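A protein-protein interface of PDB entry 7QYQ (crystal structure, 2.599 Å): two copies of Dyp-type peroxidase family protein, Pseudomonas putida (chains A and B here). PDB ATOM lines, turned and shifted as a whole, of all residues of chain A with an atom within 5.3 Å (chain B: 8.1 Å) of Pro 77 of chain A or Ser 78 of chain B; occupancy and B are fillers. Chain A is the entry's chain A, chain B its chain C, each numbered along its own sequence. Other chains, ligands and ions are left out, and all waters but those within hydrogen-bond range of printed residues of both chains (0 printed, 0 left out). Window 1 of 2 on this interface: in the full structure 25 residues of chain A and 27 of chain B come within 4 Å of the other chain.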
ATOM      1  N   PHE A  67       6.915  -1.828  -2.521  1.00  0.00           N
ATOM      2  CA  PHE A  67       6.223  -0.843  -1.702  1.00  0.00           C
ATOM      3  C   PHE A  67       6.025  -1.390  -0.292  1.00  0.00           C
ATOM      4  O   PHE A  67       5.596  -2.540  -0.133  1.00  0.00           O
ATOM      5  CB  PHE A  67       4.877  -0.485  -2.332  1.00  0.00           C
ATOM      6  CG  PHE A  67       4.197   0.689  -1.688  1.00  0.00           C
ATOM      7  CD1 PHE A  67       4.465   1.980  -2.111  1.00  0.00           C
ATOM      8  CD2 PHE A  67       3.283   0.500  -0.663  1.00  0.00           C
ATOM      9  CE1 PHE A  67       3.839   3.063  -1.520  1.00  0.00           C
ATOM     10  CE2 PHE A  67       2.654   1.576  -0.067  1.00  0.00           C
ATOM     11  CZ  PHE A  67       2.931   2.859  -0.497  1.00  0.00           C
ATOM     12  N   LEU A  69       4.901  -2.206   3.718  1.00  0.00           N
ATOM     13  CA  LEU A  69       3.666  -2.614   4.379  1.00  0.00           C
ATOM     14  C   LEU A  69       3.575  -1.879   5.711  1.00  0.00           C
ATOM     15  O   LEU A  69       4.339  -2.165   6.638  1.00  0.00           O
ATOM     16  CB  LEU A  69       3.645  -4.128   4.570  1.00  0.00           C
ATOM     17  CG  LEU A  69       2.411  -4.765   5.205  1.00  0.00           C
ATOM     18  CD1 LEU A  69       1.236  -4.730   4.244  1.00  0.00           C
ATOM     19  CD2 LEU A  69       2.730  -6.188   5.632  1.00  0.00           C
ATOM     20  N   GLU A  75      -5.099   2.913   5.671  1.00  0.00           N
ATOM     21  CA  GLU A  75      -4.827   1.910   4.651  1.00  0.00           C
ATOM     22  C   GLU A  75      -3.919   2.509   3.584  1.00  0.00           C
ATOM     23  O   GLU A  75      -4.306   3.457   2.894  1.00  0.00           O
ATOM     24  CB  GLU A  75      -6.129   1.406   4.032  1.00  0.00           C
ATOM     25  CG  GLU A  75      -7.030   0.664   5.007  1.00  0.00           C
ATOM     26  CD  GLU A  75      -8.416   0.422   4.449  1.00  0.00           C
ATOM     27  OE1 GLU A  75      -8.576   0.469   3.212  1.00  0.00           O
ATOM     28  OE2 GLU A  75      -9.344   0.189   5.249  1.00  0.00           O
ATOM     29  N   ASN A  76      -2.712   1.956   3.459  1.00  0.00           N
ATOM     30  CA  ASN A  76      -1.771   2.292   2.390  1.00  0.00           C
ATOM     31  C   ASN A  76      -1.470   1.007   1.635  1.00  0.00           C
ATOM     32  O   ASN A  76      -0.527   0.278   1.983  1.00  0.00           O
ATOM     33  CB  ASN A  76      -0.494   2.919   2.946  1.00  0.00           C
ATOM     34  CG  ASN A  76      -0.739   4.261   3.599  1.00  0.00           C
ATOM     35  OD1 ASN A  76      -0.955   5.266   2.922  1.00  0.00           O
ATOM     36  ND2 ASN A  76      -0.698   4.288   4.927  1.00  0.00           N
ATOM     37  N   PRO A  77      -2.246   0.681   0.605  1.00  0.00           N
ATOM     38  CA  PRO A  77      -2.075  -0.613  -0.067  1.00  0.00           C
ATOM     39  C   PRO A  77      -0.741  -0.712  -0.790  1.00  0.00           C
ATOM     40  O   PRO A  77      -0.162   0.286  -1.228  1.00  0.00           O
ATOM     41  CB  PRO A  77      -3.242  -0.655  -1.064  1.00  0.00           C
ATOM     42  CG  PRO A  77      -4.208   0.389  -0.587  1.00  0.00           C
ATOM     43  CD  PRO A  77      -3.372   1.450   0.050  1.00  0.00           C
ATOM     44  N   SER A  78      -0.256  -1.945  -0.909  1.00  0.00           N
ATOM     45  CA  SER A  78       0.961  -2.256  -1.648  1.00  0.00           C
ATOM     46  C   SER A  78       0.563  -3.062  -2.878  1.00  0.00           C
ATOM     47  O   SER A  78       0.232  -4.248  -2.770  1.00  0.00           O
ATOM     48  CB  SER A  78       1.956  -3.020  -0.775  1.00  0.00           C
ATOM     49  OG  SER A  78       3.193  -3.197  -1.445  1.00  0.00           O
ATOM     50  N   THR A  79       0.594  -2.422  -4.039  1.00  0.00           N
ATOM     51  CA  THR A  79       0.233  -3.051  -5.307  1.00  0.00           C
ATOM     52  C   THR A  79       1.439  -2.953  -6.238  1.00  0.00           C
ATOM     53  O   THR A  79       1.431  -2.205  -7.221  1.00  0.00           O
ATOM     54  CB  THR A  79      -1.019  -2.391  -5.912  1.00  0.00           C
ATOM     55  OG1 THR A  79      -2.041  -2.305  -4.912  1.00  0.00           O
ATOM     56  CG2 THR A  79      -1.551  -3.215  -7.075  1.00  0.00           C
ATOM     57  N   GLN A 158       1.206   6.445  -5.861  1.00  0.00           N
ATOM     58  CA  GLN A 158      -0.018   6.145  -5.128  1.00  0.00           C
ATOM     59  C   GLN A 158      -1.190   6.795  -5.843  1.00  0.00           C
ATOM     60  O   GLN A 158      -1.114   7.966  -6.226  1.00  0.00           O
ATOM     61  CB  GLN A 158       0.051   6.643  -3.678  1.00  0.00           C
ATOM     62  CG  GLN A 158       0.876   5.772  -2.740  1.00  0.00           C
ATOM     63  CD  GLN A 158       0.798   6.233  -1.294  1.00  0.00           C
ATOM     64  OE1 GLN A 158       0.895   7.425  -1.005  1.00  0.00           O
ATOM     65  NE2 GLN A 158       0.626   5.285  -0.378  1.00  0.00           N
ATOM     66  N   PRO A 263      -5.547   6.103  -0.489  1.00  0.00           N
ATOM     67  CA  PRO A 263      -4.838   5.574  -1.657  1.00  0.00           C
ATOM     68  C   PRO A 263      -5.404   4.231  -2.090  1.00  0.00           C
ATOM     69  O   PRO A 263      -5.756   3.383  -1.266  1.00  0.00           O
ATOM     70  CB  PRO A 263      -3.395   5.435  -1.158  1.00  0.00           C
ATOM     71  CG  PRO A 263      -3.542   5.192   0.303  1.00  0.00           C
ATOM     72  CD  PRO A 263      -4.751   5.981   0.745  1.00  0.00           C
ATOM     73  N   LEU A 264      -5.502   4.052  -3.407  1.00  0.00           N
ATOM     74  CA  LEU A 264      -5.975   2.800  -3.980  1.00  0.00           C
ATOM     75  C   LEU A 264      -4.843   1.873  -4.399  1.00  0.00           C
ATOM     76  O   LEU A 264      -5.045   0.654  -4.439  1.00  0.00           O
ATOM     77  CB  LEU A 264      -6.875   3.080  -5.191  1.00  0.00           C
ATOM     78  CG  LEU A 264      -8.115   3.941  -4.927  1.00  0.00           C
ATOM     79  CD1 LEU A 264      -8.923   4.154  -6.202  1.00  0.00           C
ATOM     80  CD2 LEU A 264      -8.980   3.321  -3.842  1.00  0.00           C
ATOM     81  N   THR A 265      -3.665   2.416  -4.703  1.00  0.00           N
ATOM     82  CA  THR A 265      -2.525   1.628  -5.148  1.00  0.00           C
ATOM     83  C   THR A 265      -1.278   2.096  -4.413  1.00  0.00           C
ATOM     84  O   THR A 265      -1.276   3.125  -3.731  1.00  0.00           O
ATOM     85  CB  THR A 265      -2.313   1.734  -6.668  1.00  0.00           C
ATOM     86  OG1 THR A 265      -1.949   3.077  -7.012  1.00  0.00           O
ATOM     87  CG2 THR A 265      -3.575   1.340  -7.430  1.00  0.00           C
ATOM     88  N   GLY A 266      -0.207   1.318  -4.554  1.00  0.00           N
ATOM     89  CA  GLY A 266       1.081   1.672  -3.992  1.00  0.00           C
ATOM     90  C   GLY A 266       2.215   0.943  -4.682  1.00  0.00           C
ATOM     91  O   GLY A 266       2.208  -0.290  -4.757  1.00  0.00           O
ATOM     92  N   ARG B  65      -2.293  -9.529  12.063  1.00  0.00           N
ATOM     93  CA  ARG B  65      -1.317  -8.688  11.389  1.00  0.00           C
ATOM     94  C   ARG B  65      -1.781  -8.482   9.956  1.00  0.00           C
ATOM     95  O   ARG B  65      -2.627  -9.237   9.461  1.00  0.00           O
ATOM     96  CB  ARG B  65       0.086  -9.314  11.426  1.00  0.00           C
ATOM     97  CG  ARG B  65       0.215 -10.632  10.682  1.00  0.00           C
ATOM     98  CD  ARG B  65       1.653 -11.126  10.712  1.00  0.00           C
ATOM     99  NE  ARG B  65       1.830 -12.360   9.954  1.00  0.00           N
ATOM    100  CZ  ARG B  65       1.707 -13.577  10.470  1.00  0.00           C
ATOM    101  NH1 ARG B  65       1.404 -13.729  11.751  1.00  0.00           N
ATOM    102  NH2 ARG B  65       1.887 -14.646   9.705  1.00  0.00           N
ATOM    103  N   PRO B  66      -1.264  -7.465   9.266  1.00  0.00           N
ATOM    104  CA  PRO B  66      -1.697  -7.218   7.884  1.00  0.00           C
ATOM    105  C   PRO B  66      -1.224  -8.316   6.941  1.00  0.00           C
ATOM    106  O   PRO B  66      -0.374  -9.145   7.271  1.00  0.00           O
ATOM    107  CB  PRO B  66      -1.050  -5.873   7.535  1.00  0.00           C
ATOM    108  CG  PRO B  66      -0.697  -5.253   8.847  1.00  0.00           C
ATOM    109  CD  PRO B  66      -0.384  -6.393   9.762  1.00  0.00           C
ATOM    110  N   PHE B  67      -1.820  -8.318   5.751  1.00  0.00           N
ATOM    111  CA  PHE B  67      -1.410  -9.247   4.705  1.00  0.00           C
ATOM    112  C   PHE B  67       0.065  -9.025   4.381  1.00  0.00           C
ATOM    113  O   PHE B  67       0.489  -7.873   4.213  1.00  0.00           O
ATOM    114  CB  PHE B  67      -2.265  -9.052   3.453  1.00  0.00           C
ATOM    115  CG  PHE B  67      -2.087 -10.130   2.419  1.00  0.00           C
ATOM    116  CD1 PHE B  67      -2.856 -11.282   2.464  1.00  0.00           C
ATOM    117  CD2 PHE B  67      -1.155  -9.992   1.403  1.00  0.00           C
ATOM    118  CE1 PHE B  67      -2.698 -12.276   1.517  1.00  0.00           C
ATOM    119  CE2 PHE B  67      -0.990 -10.985   0.453  1.00  0.00           C
ATOM    120  CZ  PHE B  67      -1.764 -12.127   0.511  1.00  0.00           C
ATOM    121  N   PRO B  68       0.867 -10.080   4.269  1.00  0.00           N
ATOM    122  CA  PRO B  68       2.320  -9.900   4.174  1.00  0.00           C
ATOM    123  C   PRO B  68       2.739  -9.314   2.835  1.00  0.00           C
ATOM    124  O   PRO B  68       1.966  -9.221   1.879  1.00  0.00           O
ATOM    125  CB  PRO B  68       2.859 -11.321   4.354  1.00  0.00           C
ATOM    126  CG  PRO B  68       1.770 -12.189   3.827  1.00  0.00           C
ATOM    127  CD  PRO B  68       0.484 -11.501   4.203  1.00  0.00           C
ATOM    128  N   LEU B  69       4.006  -8.908   2.788  1.00  0.00           N
ATOM    129  CA  LEU B  69       4.631  -8.342   1.597  1.00  0.00           C
ATOM    130  C   LEU B  69       5.663  -9.343   1.092  1.00  0.00           C
ATOM    131  O   LEU B  69       6.705  -9.540   1.726  1.00  0.00           O
ATOM    132  CB  LEU B  69       5.277  -6.994   1.912  1.00  0.00           C
ATOM    133  CG  LEU B  69       5.950  -6.260   0.753  1.00  0.00           C
ATOM    134  CD1 LEU B  69       4.911  -5.723  -0.214  1.00  0.00           C
ATOM    135  CD2 LEU B  69       6.844  -5.142   1.273  1.00  0.00           C
ATOM    136  N   LEU B  70       5.373  -9.971  -0.044  1.00  0.00           N
ATOM    137  CA  LEU B  70       6.227 -11.012  -0.607  1.00  0.00           C
ATOM    138  C   LEU B  70       7.058 -10.416  -1.738  1.00  0.00           C
ATOM    139  O   LEU B  70       6.521 -10.060  -2.792  1.00  0.00           O
ATOM    140  CB  LEU B  70       5.393 -12.190  -1.107  1.00  0.00           C
ATOM    141  CG  LEU B  70       5.054 -13.307  -0.115  1.00  0.00           C
ATOM    142  CD1 LEU B  70       4.176 -12.803   1.024  1.00  0.00           C
ATOM    143  CD2 LEU B  70       4.392 -14.477  -0.830  1.00  0.00           C
ATOM    144  N   GLU B  75       3.258 -11.422  -8.377  1.00  0.00           N
ATOM    145  CA  GLU B  75       2.605 -10.325  -7.674  1.00  0.00           C
ATOM    146  C   GLU B  75       1.475 -10.859  -6.802  1.00  0.00           C
ATOM    147  O   GLU B  75       0.499 -11.417  -7.313  1.00  0.00           O
ATOM    148  CB  GLU B  75       2.076  -9.289  -8.664  1.00  0.00           C
ATOM    149  CG  GLU B  75       3.167  -8.579  -9.450  1.00  0.00           C
ATOM    150  CD  GLU B  75       2.618  -7.762 -10.601  1.00  0.00           C
ATOM    151  OE1 GLU B  75       1.414  -7.431 -10.573  1.00  0.00           O
ATOM    152  OE2 GLU B  75       3.389  -7.447 -11.531  1.00  0.00           O
ATOM    153  N   ASN B  76       1.616 -10.685  -5.487  1.00  0.00           N
ATOM    154  CA  ASN B  76       0.567 -10.973  -4.512  1.00  0.00           C
ATOM    155  C   ASN B  76       0.285  -9.672  -3.771  1.00  0.00           C
ATOM    156  O   ASN B  76       0.919  -9.383  -2.743  1.00  0.00           O
ATOM    157  CB  ASN B  76       0.982 -12.086  -3.551  1.00  0.00           C
ATOM    158  CG  ASN B  76       1.149 -13.427  -4.244  1.00  0.00           C
ATOM    159  OD1 ASN B  76       0.169 -14.081  -4.601  1.00  0.00           O
ATOM    160  ND2 ASN B  76       2.396 -13.848  -4.431  1.00  0.00           N
ATOM    161  N   PRO B  77      -0.643  -8.852  -4.261  1.00  0.00           N
ATOM    162  CA  PRO B  77      -0.850  -7.530  -3.661  1.00  0.00           C
ATOM    163  C   PRO B  77      -1.391  -7.621  -2.244  1.00  0.00           C
ATOM    164  O   PRO B  77      -2.054  -8.588  -1.862  1.00  0.00           O
ATOM    165  CB  PRO B  77      -1.866  -6.870  -4.601  1.00  0.00           C
ATOM    166  CG  PRO B  77      -2.590  -8.009  -5.227  1.00  0.00           C
ATOM    167  CD  PRO B  77      -1.580  -9.115  -5.367  1.00  0.00           C
ATOM    168  N   SER B  78      -1.093  -6.587  -1.460  1.00  0.00           N
ATOM    169  CA  SER B  78      -1.577  -6.458  -0.091  1.00  0.00           C
ATOM    170  C   SER B  78      -2.584  -5.316  -0.050  1.00  0.00           C
ATOM    171  O   SER B  78      -2.204  -4.142  -0.111  1.00  0.00           O
ATOM    172  CB  SER B  78      -0.422  -6.211   0.878  1.00  0.00           C
ATOM    173  OG  SER B  78      -0.877  -6.221   2.221  1.00  0.00           O
ATOM    174  N   THR B  79      -3.861  -5.661   0.053  1.00  0.00           N
ATOM    175  CA  THR B  79      -4.949  -4.689   0.102  1.00  0.00           C
ATOM    176  C   THR B  79      -5.710  -4.901   1.409  1.00  0.00           C
ATOM    177  O   THR B  79      -6.857  -5.359   1.414  1.00  0.00           O
ATOM    178  CB  THR B  79      -5.866  -4.829  -1.128  1.00  0.00           C
ATOM    179  OG1 THR B  79      -5.068  -4.857  -2.317  1.00  0.00           O
ATOM    180  CG2 THR B  79      -6.826  -3.653  -1.219  1.00  0.00           C
ATOM    181  N   GLN B  80      -5.057  -4.578   2.522  1.00  0.00           N
ATOM    182  CA  GLN B  80      -5.632  -4.810   3.839  1.00  0.00           C
ATOM    183  C   GLN B  80      -6.648  -3.727   4.168  1.00  0.00           C
ATOM    184  O   GLN B  80      -6.369  -2.533   4.019  1.00  0.00           O
ATOM    185  CB  GLN B  80      -4.537  -4.845   4.905  1.00  0.00           C
ATOM    186  CG  GLN B  80      -5.028  -5.286   6.274  1.00  0.00           C
ATOM    187  CD  GLN B  80      -5.693  -6.646   6.245  1.00  0.00           C
ATOM    188  OE1 GLN B  80      -5.100  -7.629   5.802  1.00  0.00           O
ATOM    189  NE2 GLN B  80      -6.931  -6.711   6.722  1.00  0.00           N
ATOM    190  N   HIS B  81      -7.825  -4.146   4.615  1.00  0.00           N
ATOM    191  CA  HIS B  81      -8.894  -3.247   5.026  1.00  0.00           C
ATOM    192  C   HIS B  81      -9.189  -3.455   6.508  1.00  0.00           C
ATOM    193  O   HIS B  81      -8.634  -4.344   7.160  1.00  0.00           O
ATOM    194  CB  HIS B  81     -10.146  -3.462   4.171  1.00  0.00           C
ATOM    195  CG  HIS B  81      -9.941  -3.164   2.718  1.00  0.00           C
ATOM    196  ND1 HIS B  81      -9.577  -1.916   2.261  1.00  0.00           N
ATOM    197  CD2 HIS B  81     -10.050  -3.950   1.620  1.00  0.00           C
ATOM    198  CE1 HIS B  81      -9.471  -1.945   0.944  1.00  0.00           C
ATOM    199  NE2 HIS B  81      -9.754  -3.167   0.530  1.00  0.00           N
ATOM    200  N   PHE B 157      -7.616 -13.779   2.559  1.00  0.00           N
ATOM    201  CA  PHE B 157      -8.489 -13.595   1.408  1.00  0.00           C
ATOM    202  C   PHE B 157      -7.688 -13.114   0.207  1.00  0.00           C
ATOM    203  O   PHE B 157      -6.829 -12.236   0.332  1.00  0.00           O
ATOM    204  CB  PHE B 157      -9.610 -12.594   1.719  1.00  0.00           C
ATOM    205  CG  PHE B 157     -10.653 -12.498   0.641  1.00  0.00           C
ATOM    206  CD1 PHE B 157     -10.501 -11.616  -0.417  1.00  0.00           C
ATOM    207  CD2 PHE B 157     -11.779 -13.301   0.681  1.00  0.00           C
ATOM    208  CE1 PHE B 157     -11.459 -11.532  -1.413  1.00  0.00           C
ATOM    209  CE2 PHE B 157     -12.740 -13.223  -0.310  1.00  0.00           C
ATOM    210  CZ  PHE B 157     -12.580 -12.337  -1.359  1.00  0.00           C
ATOM    211  N   GLN B 158      -7.985 -13.691  -0.957  1.00  0.00           N
ATOM    212  CA  GLN B 158      -7.365 -13.288  -2.213  1.00  0.00           C
ATOM    213  C   GLN B 158      -8.386 -13.418  -3.333  1.00  0.00           C
ATOM    214  O   GLN B 158      -9.075 -14.438  -3.430  1.00  0.00           O
ATOM    215  CB  GLN B 158      -6.129 -14.142  -2.523  1.00  0.00           C
ATOM    216  CG  GLN B 158      -4.888 -13.773  -1.722  1.00  0.00           C
ATOM    217  CD  GLN B 158      -3.659 -14.546  -2.161  1.00  0.00           C
ATOM    218  OE1 GLN B 158      -3.714 -15.760  -2.365  1.00  0.00           O
ATOM    219  NE2 GLN B 158      -2.542 -13.845  -2.313  1.00  0.00           N
ATOM    220  N   PRO B 263      -3.588 -12.825  -8.340  1.00  0.00           N
ATOM    221  CA  PRO B 263      -4.481 -12.228  -7.340  1.00  0.00           C
ATOM    222  C   PRO B 263      -4.564 -10.718  -7.489  1.00  0.00           C
ATOM    223  O   PRO B 263      -3.568 -10.040  -7.757  1.00  0.00           O
ATOM    224  CB  PRO B 263      -3.828 -12.620  -6.010  1.00  0.00           C
ATOM    225  CG  PRO B 263      -2.373 -12.733  -6.340  1.00  0.00           C
ATOM    226  CD  PRO B 263      -2.304 -13.252  -7.756  1.00  0.00           C
ATOM    227  N   LEU B 264      -5.776 -10.194  -7.315  1.00  0.00           N
ATOM    228  CA  LEU B 264      -6.012  -8.758  -7.366  1.00  0.00           C
ATOM    229  C   LEU B 264      -6.017  -8.111  -5.990  1.00  0.00           C
ATOM    230  O   LEU B 264      -5.735  -6.913  -5.883  1.00  0.00           O
ATOM    231  CB  LEU B 264      -7.346  -8.461  -8.061  1.00  0.00           C
ATOM    232  CG  LEU B 264      -7.513  -8.960  -9.497  1.00  0.00           C
ATOM    233  CD1 LEU B 264      -8.888  -8.592 -10.033  1.00  0.00           C
ATOM    234  CD2 LEU B 264      -6.419  -8.401 -10.393  1.00  0.00           C
ATOM    235  N   THR B 265      -6.326  -8.872  -4.942  1.00  0.00           N
ATOM    236  CA  THR B 265      -6.390  -8.351  -3.586  1.00  0.00           C
ATOM    237  C   THR B 265      -5.675  -9.315  -2.651  1.00  0.00           C
ATOM    238  O   THR B 265      -5.317 -10.435  -3.027  1.00  0.00           O
ATOM    239  CB  THR B 265      -7.839  -8.144  -3.114  1.00  0.00           C
ATOM    240  OG1 THR B 265      -8.503  -9.410  -3.016  1.00  0.00           O
ATOM    241  CG2 THR B 265      -8.606  -7.240  -4.072  1.00  0.00           C
ATOM    242  N   GLY B 266      -5.459  -8.858  -1.421  1.00  0.00           N
ATOM    243  CA  GLY B 266      -4.870  -9.679  -0.383  1.00  0.00           C
ATOM    244  C   GLY B 266      -5.202  -9.137   0.991  1.00  0.00           C
ATOM    245  O   GLY B 266      -4.937  -7.966   1.277  1.00  0.00           O
ATOM    246  N   GLY B 267      -5.785  -9.969   1.852  1.00  0.00           N
ATOM    247  CA  GLY B 267      -6.179  -9.501   3.166  1.00  0.00           C
ATOM    248  C   GLY B 267      -6.122 -10.534   4.273  1.00  0.00           C
ATOM    249  O   GLY B 267      -6.452 -11.706   4.067  1.00  0.00           O
ATOM    250  N   TYR B 268      -5.703 -10.100   5.458  1.00  0.00           N
ATOM    251  CA  TYR B 268      -5.741 -10.910   6.666  1.00  0.00           C
ATOM    252  C   TYR B 268      -6.843 -10.395   7.582  1.00  0.00           C
ATOM    253  O   TYR B 268      -6.988  -9.182   7.769  1.00  0.00           O
ATOM    254  CB  TYR B 268      -4.395 -10.878   7.395  1.00  0.00           C
ATOM    255  CG  TYR B 268      -3.364 -11.853   6.865  1.00  0.00           C
ATOM    256  CD1 TYR B 268      -3.640 -12.670   5.777  1.00  0.00           C
ATOM    257  CD2 TYR B 268      -2.115 -11.965   7.464  1.00  0.00           C
ATOM    258  CE1 TYR B 268      -2.699 -13.564   5.294  1.00  0.00           C
ATOM    259  CE2 TYR B 268      -1.168 -12.857   6.992  1.00  0.00           C
ATOM    260  CZ  TYR B 268      -1.467 -13.654   5.906  1.00  0.00           C
ATOM    261  OH  TYR B 268      -0.527 -14.541   5.430  1.00  0.00           O
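Among the printed residues, merely in contact across the chains: Phe 67 of chain A with Leu 69 of chain B, Leu 69 of chain A with Phe 67 of chain B, Leu 69 of chain A with Ser 78 of chain B, Glu 75 of chain A with Gln 80 of chain B, Pro 77 of chain A with Ser 78 of chain B, Ser 78 of chain A with Leu 69 of chain B and Ser 78 of chain A with Pro 77 of chain B.
N of Gly 266 of chain B lies close to O of Pro 77 of chain B, 3.4 Å away. N of Phe 67 of chain B sits at hydrogen-bond distance from OE1 of Gln 80 of chain B (3.4 Å). OE1 of Gln 80 of chain B sits at hydrogen-bond distance from N of Tyr 268 of chain B (2.6 Å). The backbone carbonyl oxygen of Phe 67 of chain B sits at hydrogen-bond distance from the side-chain hydroxyl of Ser 78 of chain B, 2.9 Å away. OG of Ser 78 of chain A lies within hydrogen-bond range of O of Phe 67 of chain A (2.8 Å). N of Gly 266 of chain A sits close to O of Pro 77 of chain A, at 3.5 Å.
Phe 67 of chain A touches Leu 69 of chain B, and with the chains exchanged Leu 69 of chain A touches Phe 67 of chain B. Leu 69 of chain A touches Ser 78 of chain B, and with the chains exchanged Ser 78 of chain A touches Leu 69 of chain B. Pro 77 of chain A touches Ser 78 of chain B, and with the chains exchanged Ser 78 of chain A touches Pro 77 of chain B. Ser 78 of chain B touches its own counterpart, Ser 78 of chain A. Positions printed for both chains: 67, 69, 75, 76, 77, 78, 79, 158, 263, 264, 265 and 266. Of the 9 pairs that touch across the chains among the printed residues, 7 have their exchanged pair printed and touching as well.
Of the 21 printed residues of chain B, 6 touch a printed residue of chain A. Hydrophobic or aromatic side chains of chain B that line the printed part of chain A: Leu 69, Pro 77 and His 81. Among the printed residues, 9 pairs touch across the chains.
Of the printed residues of chain B, Glu 75 of chain A touches Gln 80 and His 81. Of the printed residues of chain B, Ser 78 of chain A touches Leu 69 (3.3 Å), Pro 77 (3.6 Å) and Ser 78 (3.0 Å). Of the printed residues of chain A, Ser 78 of chain B touches Leu 69, Pro 77 and Ser 78. Gln 158 of chain B touches none of the printed residues of chain A. The nearest residue of chain B that does not touch Pro 77 of chain A is Thr 79 of chain B (4.5 Å). The nearest printed residue of chain B that does not touch Glu 75 of chain A is Thr 79 of chain B (6.3 Å).
OE1 of Glu 75 of chain A is in hydrogen-bond range of ND1 of His 81 of chain B, 2.8 Å away. O of Ser 78 of chain A is in hydrogen-bond range of N of Ser 78 of chain B (3.0 Å).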
